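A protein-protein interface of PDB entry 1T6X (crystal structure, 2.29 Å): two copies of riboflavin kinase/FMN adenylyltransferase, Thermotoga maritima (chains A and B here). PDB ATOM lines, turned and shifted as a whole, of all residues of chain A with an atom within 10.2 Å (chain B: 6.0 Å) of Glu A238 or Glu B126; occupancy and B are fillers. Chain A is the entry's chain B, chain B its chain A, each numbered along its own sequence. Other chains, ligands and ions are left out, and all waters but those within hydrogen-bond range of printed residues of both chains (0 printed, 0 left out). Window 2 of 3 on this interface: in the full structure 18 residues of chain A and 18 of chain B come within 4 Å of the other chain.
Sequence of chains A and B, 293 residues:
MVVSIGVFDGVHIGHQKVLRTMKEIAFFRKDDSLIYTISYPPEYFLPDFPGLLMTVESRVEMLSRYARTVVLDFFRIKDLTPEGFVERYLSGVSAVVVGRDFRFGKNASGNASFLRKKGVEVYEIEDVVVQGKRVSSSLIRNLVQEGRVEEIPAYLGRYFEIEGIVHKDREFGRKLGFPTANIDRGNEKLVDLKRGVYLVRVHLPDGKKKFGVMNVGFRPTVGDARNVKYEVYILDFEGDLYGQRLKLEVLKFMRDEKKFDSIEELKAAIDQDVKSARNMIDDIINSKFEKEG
The guanidinium group (NH2) of Arg B134 lies within hydrogen-bond range of the backbone carbonyl oxygen (O) of Glu A238, at 2.5 Å. NE of Arg B100 is in salt-bridge range of OE1 of Glu A238 (3.7 Å).
The backbone carbonyl oxygen of Asp A236 lies within hydrogen-bond range of the side-chain amino group of Lys A210. The guanidinium group (NH1) of Arg B100 is in salt-bridge range of the side-chain carboxylate (OE1) of Glu B124, 3.7 Å away.
Among the printed residues, pairs that only touch across the chains: Asp A236 with Asp B101, Phe A237 with Asp B101, Glu A238 with Asp B101, Glu A238 with Glu B126 and Gly A239 with Arg B134.
Of the printed residues of chain B, Glu A238 touches Arg B100 (3.5 Å), Asp B101 (3.7 Å), Glu B126 (3.97 Å) and Arg B134 (2.5 Å). No residue of chain A comes within 4 Å of Ile B125. No residue of chain A comes within 4 Å of Asp B127. Of the printed residues of chain B, Phe A237 touches Asp B101 (3.9 Å). Of the printed residues of chain A, Asp B101 touches Asp A236 (3.6 Å), Phe A237 (3.9 Å) and Glu A238 (3.7 Å). Printed residues of chain B within 4 Å of Gly A239: Arg B134. Of the printed residues of chain B, Asp A236 touches Asp B101 (3.6 Å). The nearest residue of chain B that does not touch Glu A238 is Asp B127 (5.5 Å). The nearest residue of chain A that does not touch Glu B126 is Gly A239 (9.2 Å).
Of the 11 printed residues of chain B, 4 touch a printed residue of chain A. Printed residues of chain B that touch a printed residue of chain A: Arg B100, Asp B101, Glu B126 and Arg B134. Of the 18 printed residues of chain A, 4 touch a printed residue of chain B. Printed residues of chain A that touch a printed residue of chain B: Asp A236, Phe A237, Glu A238 and Gly A239.
No position is printed for both chains.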
ATOM      1  N   PHE A 178      -8.047 -25.350 -26.223  1.00  0.00           N
ATOM      2  CA  PHE A 178      -9.009 -24.743 -27.137  1.00  0.00           C
ATOM      3  C   PHE A 178      -9.628 -23.458 -26.534  1.00  0.00           C
ATOM      4  O   PHE A 178      -8.922 -22.708 -25.855  1.00  0.00           O
ATOM      5  CB  PHE A 178     -10.060 -25.792 -27.522  1.00  0.00           C
ATOM      6  CG  PHE A 178      -9.637 -26.688 -28.660  1.00  0.00           C
ATOM      7  CD1 PHE A 178      -8.530 -27.526 -28.538  1.00  0.00           C
ATOM      8  CD2 PHE A 178     -10.346 -26.692 -29.859  1.00  0.00           C
ATOM      9  CE1 PHE A 178      -8.132 -28.357 -29.595  1.00  0.00           C
ATOM     10  CE2 PHE A 178      -9.956 -27.518 -30.922  1.00  0.00           C
ATOM     11  CZ  PHE A 178      -8.848 -28.353 -30.787  1.00  0.00           C
ATOM     12  N   PRO A 179     -10.930 -23.168 -26.776  1.00  0.00           N
ATOM     13  CA  PRO A 179     -11.478 -21.936 -26.190  1.00  0.00           C
ATOM     14  C   PRO A 179     -11.230 -21.696 -24.706  1.00  0.00           C
ATOM     15  O   PRO A 179     -11.273 -22.620 -23.905  1.00  0.00           O
ATOM     16  CB  PRO A 179     -12.964 -22.048 -26.503  1.00  0.00           C
ATOM     17  CG  PRO A 179     -12.945 -22.653 -27.850  1.00  0.00           C
ATOM     18  CD  PRO A 179     -11.925 -23.769 -27.687  1.00  0.00           C
ATOM     19  N   LEU A 204     -20.786 -22.118 -13.042  1.00  0.00           N
ATOM     20  CA  LEU A 204     -21.424 -21.470 -14.187  1.00  0.00           C
ATOM     21  C   LEU A 204     -22.731 -20.825 -13.755  1.00  0.00           C
ATOM     22  O   LEU A 204     -23.221 -21.087 -12.655  1.00  0.00           O
ATOM     23  CB  LEU A 204     -21.701 -22.490 -15.306  1.00  0.00           C
ATOM     24  CG  LEU A 204     -20.534 -23.326 -15.840  1.00  0.00           C
ATOM     25  CD1 LEU A 204     -21.050 -24.351 -16.842  1.00  0.00           C
ATOM     26  CD2 LEU A 204     -19.515 -22.424 -16.478  1.00  0.00           C
ATOM     27  N   PRO A 205     -23.309 -19.971 -14.621  1.00  0.00           N
ATOM     28  CA  PRO A 205     -24.573 -19.276 -14.344  1.00  0.00           C
ATOM     29  C   PRO A 205     -25.695 -20.236 -13.938  1.00  0.00           C
ATOM     30  O   PRO A 205     -26.323 -20.063 -12.892  1.00  0.00           O
ATOM     31  CB  PRO A 205     -24.872 -18.562 -15.667  1.00  0.00           C
ATOM     32  CG  PRO A 205     -23.503 -18.260 -16.209  1.00  0.00           C
ATOM     33  CD  PRO A 205     -22.734 -19.533 -15.910  1.00  0.00           C
ATOM     34  N   ASP A 206     -25.939 -21.244 -14.772  1.00  0.00           N
ATOM     35  CA  ASP A 206     -26.986 -22.235 -14.518  1.00  0.00           C
ATOM     36  C   ASP A 206     -27.040 -22.569 -13.037  1.00  0.00           C
ATOM     37  O   ASP A 206     -28.081 -22.477 -12.386  1.00  0.00           O
ATOM     38  CB  ASP A 206     -26.707 -23.545 -15.272  1.00  0.00           C
ATOM     39  CG  ASP A 206     -26.093 -23.328 -16.636  1.00  0.00           C
ATOM     40  OD1 ASP A 206     -24.989 -22.743 -16.725  1.00  0.00           O
ATOM     41  OD2 ASP A 206     -26.714 -23.759 -17.624  1.00  0.00           O
ATOM     42  N   LYS A 208     -24.399 -24.823 -12.437  1.00  0.00           N
ATOM     43  CA  LYS A 208     -23.616 -25.985 -12.794  1.00  0.00           C
ATOM     44  C   LYS A 208     -22.170 -25.773 -12.375  1.00  0.00           C
ATOM     45  O   LYS A 208     -21.666 -24.642 -12.416  1.00  0.00           O
ATOM     46  CB  LYS A 208     -23.697 -26.184 -14.310  1.00  0.00           C
ATOM     47  CG  LYS A 208     -22.987 -27.412 -14.858  1.00  0.00           C
ATOM     48  CD  LYS A 208     -22.905 -27.354 -16.395  1.00  0.00           C
ATOM     49  CE  LYS A 208     -24.282 -27.407 -17.073  1.00  0.00           C
ATOM     50  NZ  LYS A 208     -24.907 -28.760 -16.966  1.00  0.00           N
ATOM     51  N   LYS A 210     -18.229 -27.198 -13.071  1.00  0.00           N
ATOM     52  CA  LYS A 210     -17.300 -27.985 -13.868  1.00  0.00           C
ATOM     53  C   LYS A 210     -15.945 -27.656 -13.293  1.00  0.00           C
ATOM     54  O   LYS A 210     -15.859 -26.913 -12.332  1.00  0.00           O
ATOM     55  CB  LYS A 210     -17.330 -27.559 -15.340  1.00  0.00           C
ATOM     56  CG  LYS A 210     -18.633 -27.860 -16.084  1.00  0.00           C
ATOM     57  CD  LYS A 210     -19.103 -29.273 -15.785  1.00  0.00           C
ATOM     58  CE  LYS A 210     -20.281 -29.689 -16.638  1.00  0.00           C
ATOM     59  NZ  LYS A 210     -19.843 -30.331 -17.901  1.00  0.00           N
ATOM     60  N   PHE A 211     -14.890 -28.226 -13.859  1.00  0.00           N
ATOM     61  CA  PHE A 211     -13.543 -27.938 -13.418  1.00  0.00           C
ATOM     62  C   PHE A 211     -12.929 -27.204 -14.594  1.00  0.00           C
ATOM     63  O   PHE A 211     -13.434 -27.292 -15.710  1.00  0.00           O
ATOM     64  CB  PHE A 211     -12.778 -29.222 -13.130  1.00  0.00           C
ATOM     65  CG  PHE A 211     -13.152 -29.881 -11.821  1.00  0.00           C
ATOM     66  CD1 PHE A 211     -12.437 -29.603 -10.655  1.00  0.00           C
ATOM     67  CD2 PHE A 211     -14.213 -30.790 -11.757  1.00  0.00           C
ATOM     68  CE1 PHE A 211     -12.777 -30.232  -9.436  1.00  0.00           C
ATOM     69  CE2 PHE A 211     -14.563 -31.417 -10.557  1.00  0.00           C
ATOM     70  CZ  PHE A 211     -13.847 -31.142  -9.394  1.00  0.00           C
ATOM     71  N   TYR A 233     -10.138 -22.400 -19.231  1.00  0.00           N
ATOM     72  CA  TYR A 233     -10.636 -23.378 -20.180  1.00  0.00           C
ATOM     73  C   TYR A 233     -11.447 -24.338 -19.336  1.00  0.00           C
ATOM     74  O   TYR A 233     -10.905 -25.058 -18.492  1.00  0.00           O
ATOM     75  CB  TYR A 233      -9.476 -24.114 -20.880  1.00  0.00           C
ATOM     76  CG  TYR A 233      -9.908 -25.325 -21.703  1.00  0.00           C
ATOM     77  CD1 TYR A 233     -10.902 -25.217 -22.684  1.00  0.00           C
ATOM     78  CD2 TYR A 233      -9.363 -26.588 -21.461  1.00  0.00           C
ATOM     79  CE1 TYR A 233     -11.345 -26.336 -23.396  1.00  0.00           C
ATOM     80  CE2 TYR A 233      -9.797 -27.708 -22.163  1.00  0.00           C
ATOM     81  CZ  TYR A 233     -10.789 -27.579 -23.123  1.00  0.00           C
ATOM     82  OH  TYR A 233     -11.249 -28.695 -23.781  1.00  0.00           O
ATOM     83  N   ILE A 234     -12.751 -24.338 -19.550  1.00  0.00           N
ATOM     84  CA  ILE A 234     -13.629 -25.193 -18.786  1.00  0.00           C
ATOM     85  C   ILE A 234     -13.710 -26.587 -19.406  1.00  0.00           C
ATOM     86  O   ILE A 234     -13.944 -26.730 -20.607  1.00  0.00           O
ATOM     87  CB  ILE A 234     -15.008 -24.543 -18.686  1.00  0.00           C
ATOM     88  CG1 ILE A 234     -14.821 -23.069 -18.293  1.00  0.00           C
ATOM     89  CG2 ILE A 234     -15.861 -25.274 -17.647  1.00  0.00           C
ATOM     90  CD1 ILE A 234     -16.057 -22.193 -18.404  1.00  0.00           C
ATOM     91  N   LEU A 235     -13.489 -27.611 -18.584  1.00  0.00           N
ATOM     92  CA  LEU A 235     -13.506 -28.995 -19.060  1.00  0.00           C
ATOM     93  C   LEU A 235     -14.897 -29.558 -19.306  1.00  0.00           C
ATOM     94  O   LEU A 235     -15.861 -29.254 -18.597  1.00  0.00           O
ATOM     95  CB  LEU A 235     -12.781 -29.933 -18.074  1.00  0.00           C
ATOM     96  CG  LEU A 235     -11.253 -29.910 -18.002  1.00  0.00           C
ATOM     97  CD1 LEU A 235     -10.829 -29.535 -16.584  1.00  0.00           C
ATOM     98  CD2 LEU A 235     -10.677 -31.280 -18.386  1.00  0.00           C
ATOM     99  N   ASP A 236     -14.993 -30.398 -20.327  1.00  0.00           N
ATOM    100  CA  ASP A 236     -16.253 -31.044 -20.637  1.00  0.00           C
ATOM    101  C   ASP A 236     -17.389 -30.038 -20.693  1.00  0.00           C
ATOM    102  O   ASP A 236     -18.482 -30.272 -20.162  1.00  0.00           O
ATOM    103  CB  ASP A 236     -16.514 -32.117 -19.578  1.00  0.00           C
ATOM    104  CG  ASP A 236     -15.331 -33.061 -19.423  1.00  0.00           C
ATOM    105  OD1 ASP A 236     -15.122 -33.589 -18.319  1.00  0.00           O
ATOM    106  OD2 ASP A 236     -14.609 -33.270 -20.416  1.00  0.00           O
ATOM    107  N   PHE A 237     -17.117 -28.925 -21.361  1.00  0.00           N
ATOM    108  CA  PHE A 237     -18.090 -27.857 -21.522  1.00  0.00           C
ATOM    109  C   PHE A 237     -18.092 -27.291 -22.940  1.00  0.00           C
ATOM    110  O   PHE A 237     -17.046 -27.202 -23.599  1.00  0.00           O
ATOM    111  CB  PHE A 237     -17.790 -26.719 -20.543  1.00  0.00           C
ATOM    112  CG  PHE A 237     -18.766 -25.573 -20.632  1.00  0.00           C
ATOM    113  CD1 PHE A 237     -20.018 -25.660 -20.035  1.00  0.00           C
ATOM    114  CD2 PHE A 237     -18.454 -24.433 -21.368  1.00  0.00           C
ATOM    115  CE1 PHE A 237     -20.952 -24.636 -20.171  1.00  0.00           C
ATOM    116  CE2 PHE A 237     -19.378 -23.408 -21.511  1.00  0.00           C
ATOM    117  CZ  PHE A 237     -20.635 -23.511 -20.909  1.00  0.00           C
ATOM    118  N   GLU A 238     -19.276 -26.903 -23.402  1.00  0.00           N
ATOM    119  CA  GLU A 238     -19.445 -26.301 -24.722  1.00  0.00           C
ATOM    120  C   GLU A 238     -20.507 -25.227 -24.533  1.00  0.00           C
ATOM    121  O   GLU A 238     -21.547 -25.501 -23.944  1.00  0.00           O
ATOM    122  CB  GLU A 238     -19.941 -27.331 -25.741  1.00  0.00           C
ATOM    123  CG  GLU A 238     -21.269 -27.988 -25.366  1.00  0.00           C
ATOM    124  CD  GLU A 238     -21.963 -28.653 -26.548  1.00  0.00           C
ATOM    125  OE1 GLU A 238     -23.032 -29.270 -26.341  1.00  0.00           O
ATOM    126  OE2 GLU A 238     -21.445 -28.553 -27.683  1.00  0.00           O
ATOM    127  N   GLY A 239     -20.248 -24.007 -24.998  1.00  0.00           N
ATOM    128  CA  GLY A 239     -21.238 -22.951 -24.853  1.00  0.00           C
ATOM    129  C   GLY A 239     -20.632 -21.561 -24.870  1.00  0.00           C
ATOM    130  O   GLY A 239     -19.457 -21.395 -24.547  1.00  0.00           O
ATOM    131  N   ASP A 240     -21.415 -20.563 -25.264  1.00  0.00           N
ATOM    132  CA  ASP A 240     -20.902 -19.199 -25.291  1.00  0.00           C
ATOM    133  C   ASP A 240     -21.232 -18.594 -23.932  1.00  0.00           C
ATOM    134  O   ASP A 240     -22.337 -18.765 -23.419  1.00  0.00           O
ATOM    135  CB  ASP A 240     -21.542 -18.395 -26.434  1.00  0.00           C
ATOM    136  CG  ASP A 240     -22.606 -17.425 -25.954  1.00  0.00           C
ATOM    137  OD1 ASP A 240     -23.585 -17.879 -25.324  1.00  0.00           O
ATOM    138  OD2 ASP A 240     -22.460 -16.207 -26.215  1.00  0.00           O
ATOM    139  N   LEU A 241     -20.268 -17.896 -23.344  1.00  0.00           N
ATOM    140  CA  LEU A 241     -20.462 -17.313 -22.022  1.00  0.00           C
ATOM    141  C   LEU A 241     -20.262 -15.803 -21.932  1.00  0.00           C
ATOM    142  O   LEU A 241     -20.106 -15.270 -20.829  1.00  0.00           O
ATOM    143  CB  LEU A 241     -19.520 -17.994 -21.024  1.00  0.00           C
ATOM    144  CG  LEU A 241     -19.702 -19.494 -20.790  1.00  0.00           C
ATOM    145  CD1 LEU A 241     -18.553 -20.056 -19.947  1.00  0.00           C
ATOM    146  CD2 LEU A 241     -21.055 -19.718 -20.121  1.00  0.00           C
ATOM    147  N   GLN A 244     -21.477 -13.257 -19.256  1.00  0.00           N
ATOM    148  CA  GLN A 244     -21.932 -14.099 -18.151  1.00  0.00           C
ATOM    149  C   GLN A 244     -20.952 -14.050 -16.986  1.00  0.00           C
ATOM    150  O   GLN A 244     -19.752 -13.908 -17.183  1.00  0.00           O
ATOM    151  CB  GLN A 244     -22.127 -15.539 -18.637  1.00  0.00           C
ATOM    152  CG  GLN A 244     -23.002 -15.622 -19.863  1.00  0.00           C
ATOM    153  CD  GLN A 244     -24.106 -16.633 -19.724  1.00  0.00           C
ATOM    154  OE1 GLN A 244     -24.022 -17.743 -20.258  1.00  0.00           O
ATOM    155  NE2 GLN A 244     -25.159 -16.260 -18.997  1.00  0.00           N
ATOM    156  N   GLY B  14     -34.484 -33.203 -20.489  1.00  0.00           N
ATOM    157  CA  GLY B  14     -33.329 -33.435 -21.337  1.00  0.00           C
ATOM    158  C   GLY B  14     -33.010 -34.939 -21.338  1.00  0.00           C
ATOM    159  O   GLY B  14     -32.592 -35.496 -22.342  1.00  0.00           O
ATOM    160  N   LYS B  17     -35.237 -36.822 -23.473  1.00  0.00           N
ATOM    161  CA  LYS B  17     -34.856 -36.623 -24.843  1.00  0.00           C
ATOM    162  C   LYS B  17     -33.899 -37.763 -25.200  1.00  0.00           C
ATOM    163  O   LYS B  17     -34.096 -38.451 -26.193  1.00  0.00           O
ATOM    164  CB  LYS B  17     -34.178 -35.279 -24.998  1.00  0.00           C
ATOM    165  CG  LYS B  17     -33.446 -35.089 -26.302  1.00  0.00           C
ATOM    166  CD  LYS B  17     -34.399 -34.789 -27.437  1.00  0.00           C
ATOM    167  CE  LYS B  17     -33.627 -34.681 -28.755  1.00  0.00           C
ATOM    168  NZ  LYS B  17     -32.480 -33.719 -28.668  1.00  0.00           N
ATOM    169  N   VAL B  98     -25.523 -41.173 -25.597  1.00  0.00           N
ATOM    170  CA  VAL B  98     -25.115 -40.366 -24.445  1.00  0.00           C
ATOM    171  C   VAL B  98     -25.282 -38.855 -24.691  1.00  0.00           C
ATOM    172  O   VAL B  98     -25.397 -38.404 -25.838  1.00  0.00           O
ATOM    173  CB  VAL B  98     -23.626 -40.599 -24.085  1.00  0.00           C
ATOM    174  CG1 VAL B  98     -23.397 -42.049 -23.750  1.00  0.00           C
ATOM    175  CG2 VAL B  98     -22.727 -40.196 -25.246  1.00  0.00           C
ATOM    176  N   ARG B 100     -23.951 -34.884 -24.490  1.00  0.00           N
ATOM    177  CA  ARG B 100     -22.690 -34.297 -24.931  1.00  0.00           C
ATOM    178  C   ARG B 100     -21.642 -34.364 -23.814  1.00  0.00           C
ATOM    179  O   ARG B 100     -21.982 -34.478 -22.638  1.00  0.00           O
ATOM    180  CB  ARG B 100     -22.914 -32.838 -25.316  1.00  0.00           C
ATOM    181  CG  ARG B 100     -23.969 -32.617 -26.375  1.00  0.00           C
ATOM    182  CD  ARG B 100     -23.443 -33.026 -27.713  1.00  0.00           C
ATOM    183  NE  ARG B 100     -22.122 -32.454 -27.919  1.00  0.00           N
ATOM    184  CZ  ARG B 100     -21.413 -32.605 -29.028  1.00  0.00           C
ATOM    185  NH1 ARG B 100     -21.905 -33.315 -30.038  1.00  0.00           N
ATOM    186  NH2 ARG B 100     -20.210 -32.054 -29.125  1.00  0.00           N
ATOM    187  N   ASP B 101     -20.369 -34.295 -24.189  1.00  0.00           N
ATOM    188  CA  ASP B 101     -19.268 -34.328 -23.230  1.00  0.00           C
ATOM    189  C   ASP B 101     -19.319 -35.498 -22.229  1.00  0.00           C
ATOM    190  O   ASP B 101     -18.896 -35.380 -21.075  1.00  0.00           O
ATOM    191  CB  ASP B 101     -19.196 -32.984 -22.479  1.00  0.00           C
ATOM    192  CG  ASP B 101     -19.061 -31.774 -23.427  1.00  0.00           C
ATOM    193  OD1 ASP B 101     -20.026 -30.977 -23.514  1.00  0.00           O
ATOM    194  OD2 ASP B 101     -17.995 -31.617 -24.075  1.00  0.00           O
ATOM    195  N   GLU B 124     -24.576 -38.796 -29.834  1.00  0.00           N
ATOM    196  CA  GLU B 124     -24.481 -37.723 -28.849  1.00  0.00           C
ATOM    197  C   GLU B 124     -25.679 -36.791 -28.909  1.00  0.00           C
ATOM    198  O   GLU B 124     -25.767 -35.956 -29.800  1.00  0.00           O
ATOM    199  CB  GLU B 124     -23.199 -36.938 -29.082  1.00  0.00           C
ATOM    200  CG  GLU B 124     -21.981 -37.832 -28.999  1.00  0.00           C
ATOM    201  CD  GLU B 124     -20.686 -37.078 -28.861  1.00  0.00           C
ATOM    202  OE1 GLU B 124     -20.169 -36.554 -29.877  1.00  0.00           O
ATOM    203  OE2 GLU B 124     -20.183 -37.011 -27.717  1.00  0.00           O
ATOM    204  N   ILE B 125     -26.599 -36.928 -27.964  1.00  0.00           N
ATOM    205  CA  ILE B 125     -27.798 -36.091 -27.947  1.00  0.00           C
ATOM    206  C   ILE B 125     -27.583 -34.657 -27.442  1.00  0.00           C
ATOM    207  O   ILE B 125     -26.966 -34.448 -26.397  1.00  0.00           O
ATOM    208  CB  ILE B 125     -28.869 -36.721 -27.073  1.00  0.00           C
ATOM    209  CG1 ILE B 125     -28.967 -38.215 -27.385  1.00  0.00           C
ATOM    210  CG2 ILE B 125     -30.171 -35.996 -27.247  1.00  0.00           C
ATOM    211  CD1 ILE B 125     -29.009 -38.543 -28.828  1.00  0.00           C
ATOM    212  N   GLU B 126     -28.097 -33.679 -28.186  1.00  0.00           N
ATOM    213  CA  GLU B 126     -27.971 -32.278 -27.796  1.00  0.00           C
ATOM    214  C   GLU B 126     -28.845 -31.977 -26.574  1.00  0.00           C
ATOM    215  O   GLU B 126     -29.964 -32.495 -26.454  1.00  0.00           O
ATOM    216  CB  GLU B 126     -28.405 -31.357 -28.940  1.00  0.00           C
ATOM    217  CG  GLU B 126     -27.515 -31.400 -30.149  1.00  0.00           C
ATOM    218  CD  GLU B 126     -26.149 -30.820 -29.888  1.00  0.00           C
ATOM    219  OE1 GLU B 126     -25.243 -31.024 -30.727  1.00  0.00           O
ATOM    220  OE2 GLU B 126     -25.983 -30.153 -28.845  1.00  0.00           O
ATOM    221  N   ASP B 127     -28.341 -31.134 -25.672  1.00  0.00           N
ATOM    222  CA  ASP B 127     -29.119 -30.754 -24.481  1.00  0.00           C
ATOM    223  C   ASP B 127     -30.385 -29.986 -24.882  1.00  0.00           C
ATOM    224  O   ASP B 127     -30.388 -29.233 -25.861  1.00  0.00           O
ATOM    225  CB  ASP B 127     -28.289 -29.851 -23.556  1.00  0.00           C
ATOM    226  CG  ASP B 127     -27.224 -30.606 -22.786  1.00  0.00           C
ATOM    227  OD1 ASP B 127     -26.407 -29.941 -22.110  1.00  0.00           O
ATOM    228  OD2 ASP B 127     -27.205 -31.855 -22.846  1.00  0.00           O
ATOM    229  N   VAL B 128     -31.458 -30.189 -24.131  1.00  0.00           N
ATOM    230  CA  VAL B 128     -32.698 -29.474 -24.384  1.00  0.00           C
ATOM    231  C   VAL B 128     -32.587 -28.106 -23.702  1.00  0.00           C
ATOM    232  O   VAL B 128     -32.114 -28.009 -22.566  1.00  0.00           O
ATOM    233  CB  VAL B 128     -33.901 -30.196 -23.771  1.00  0.00           C
ATOM    234  CG1 VAL B 128     -35.181 -29.397 -24.041  1.00  0.00           C
ATOM    235  CG2 VAL B 128     -34.018 -31.592 -24.343  1.00  0.00           C
ATOM    236  N   ARG B 134     -30.102 -24.435 -20.400  1.00  0.00           N
ATOM    237  CA  ARG B 134     -29.934 -25.856 -20.717  1.00  0.00           C
ATOM    238  C   ARG B 134     -30.460 -26.687 -19.579  1.00  0.00           C
ATOM    239  O   ARG B 134     -30.010 -26.546 -18.434  1.00  0.00           O
ATOM    240  CB  ARG B 134     -28.478 -26.234 -20.884  1.00  0.00           C
ATOM    241  CG  ARG B 134     -27.861 -25.817 -22.148  1.00  0.00           C
ATOM    242  CD  ARG B 134     -26.451 -26.295 -22.129  1.00  0.00           C
ATOM    243  NE  ARG B 134     -25.755 -25.776 -23.284  1.00  0.00           N
ATOM    244  CZ  ARG B 134     -24.444 -25.842 -23.457  1.00  0.00           C
ATOM    245  NH1 ARG B 134     -23.670 -26.414 -22.539  1.00  0.00           N
ATOM    246  NH2 ARG B 134     -23.914 -25.318 -24.553  1.00  0.00           N
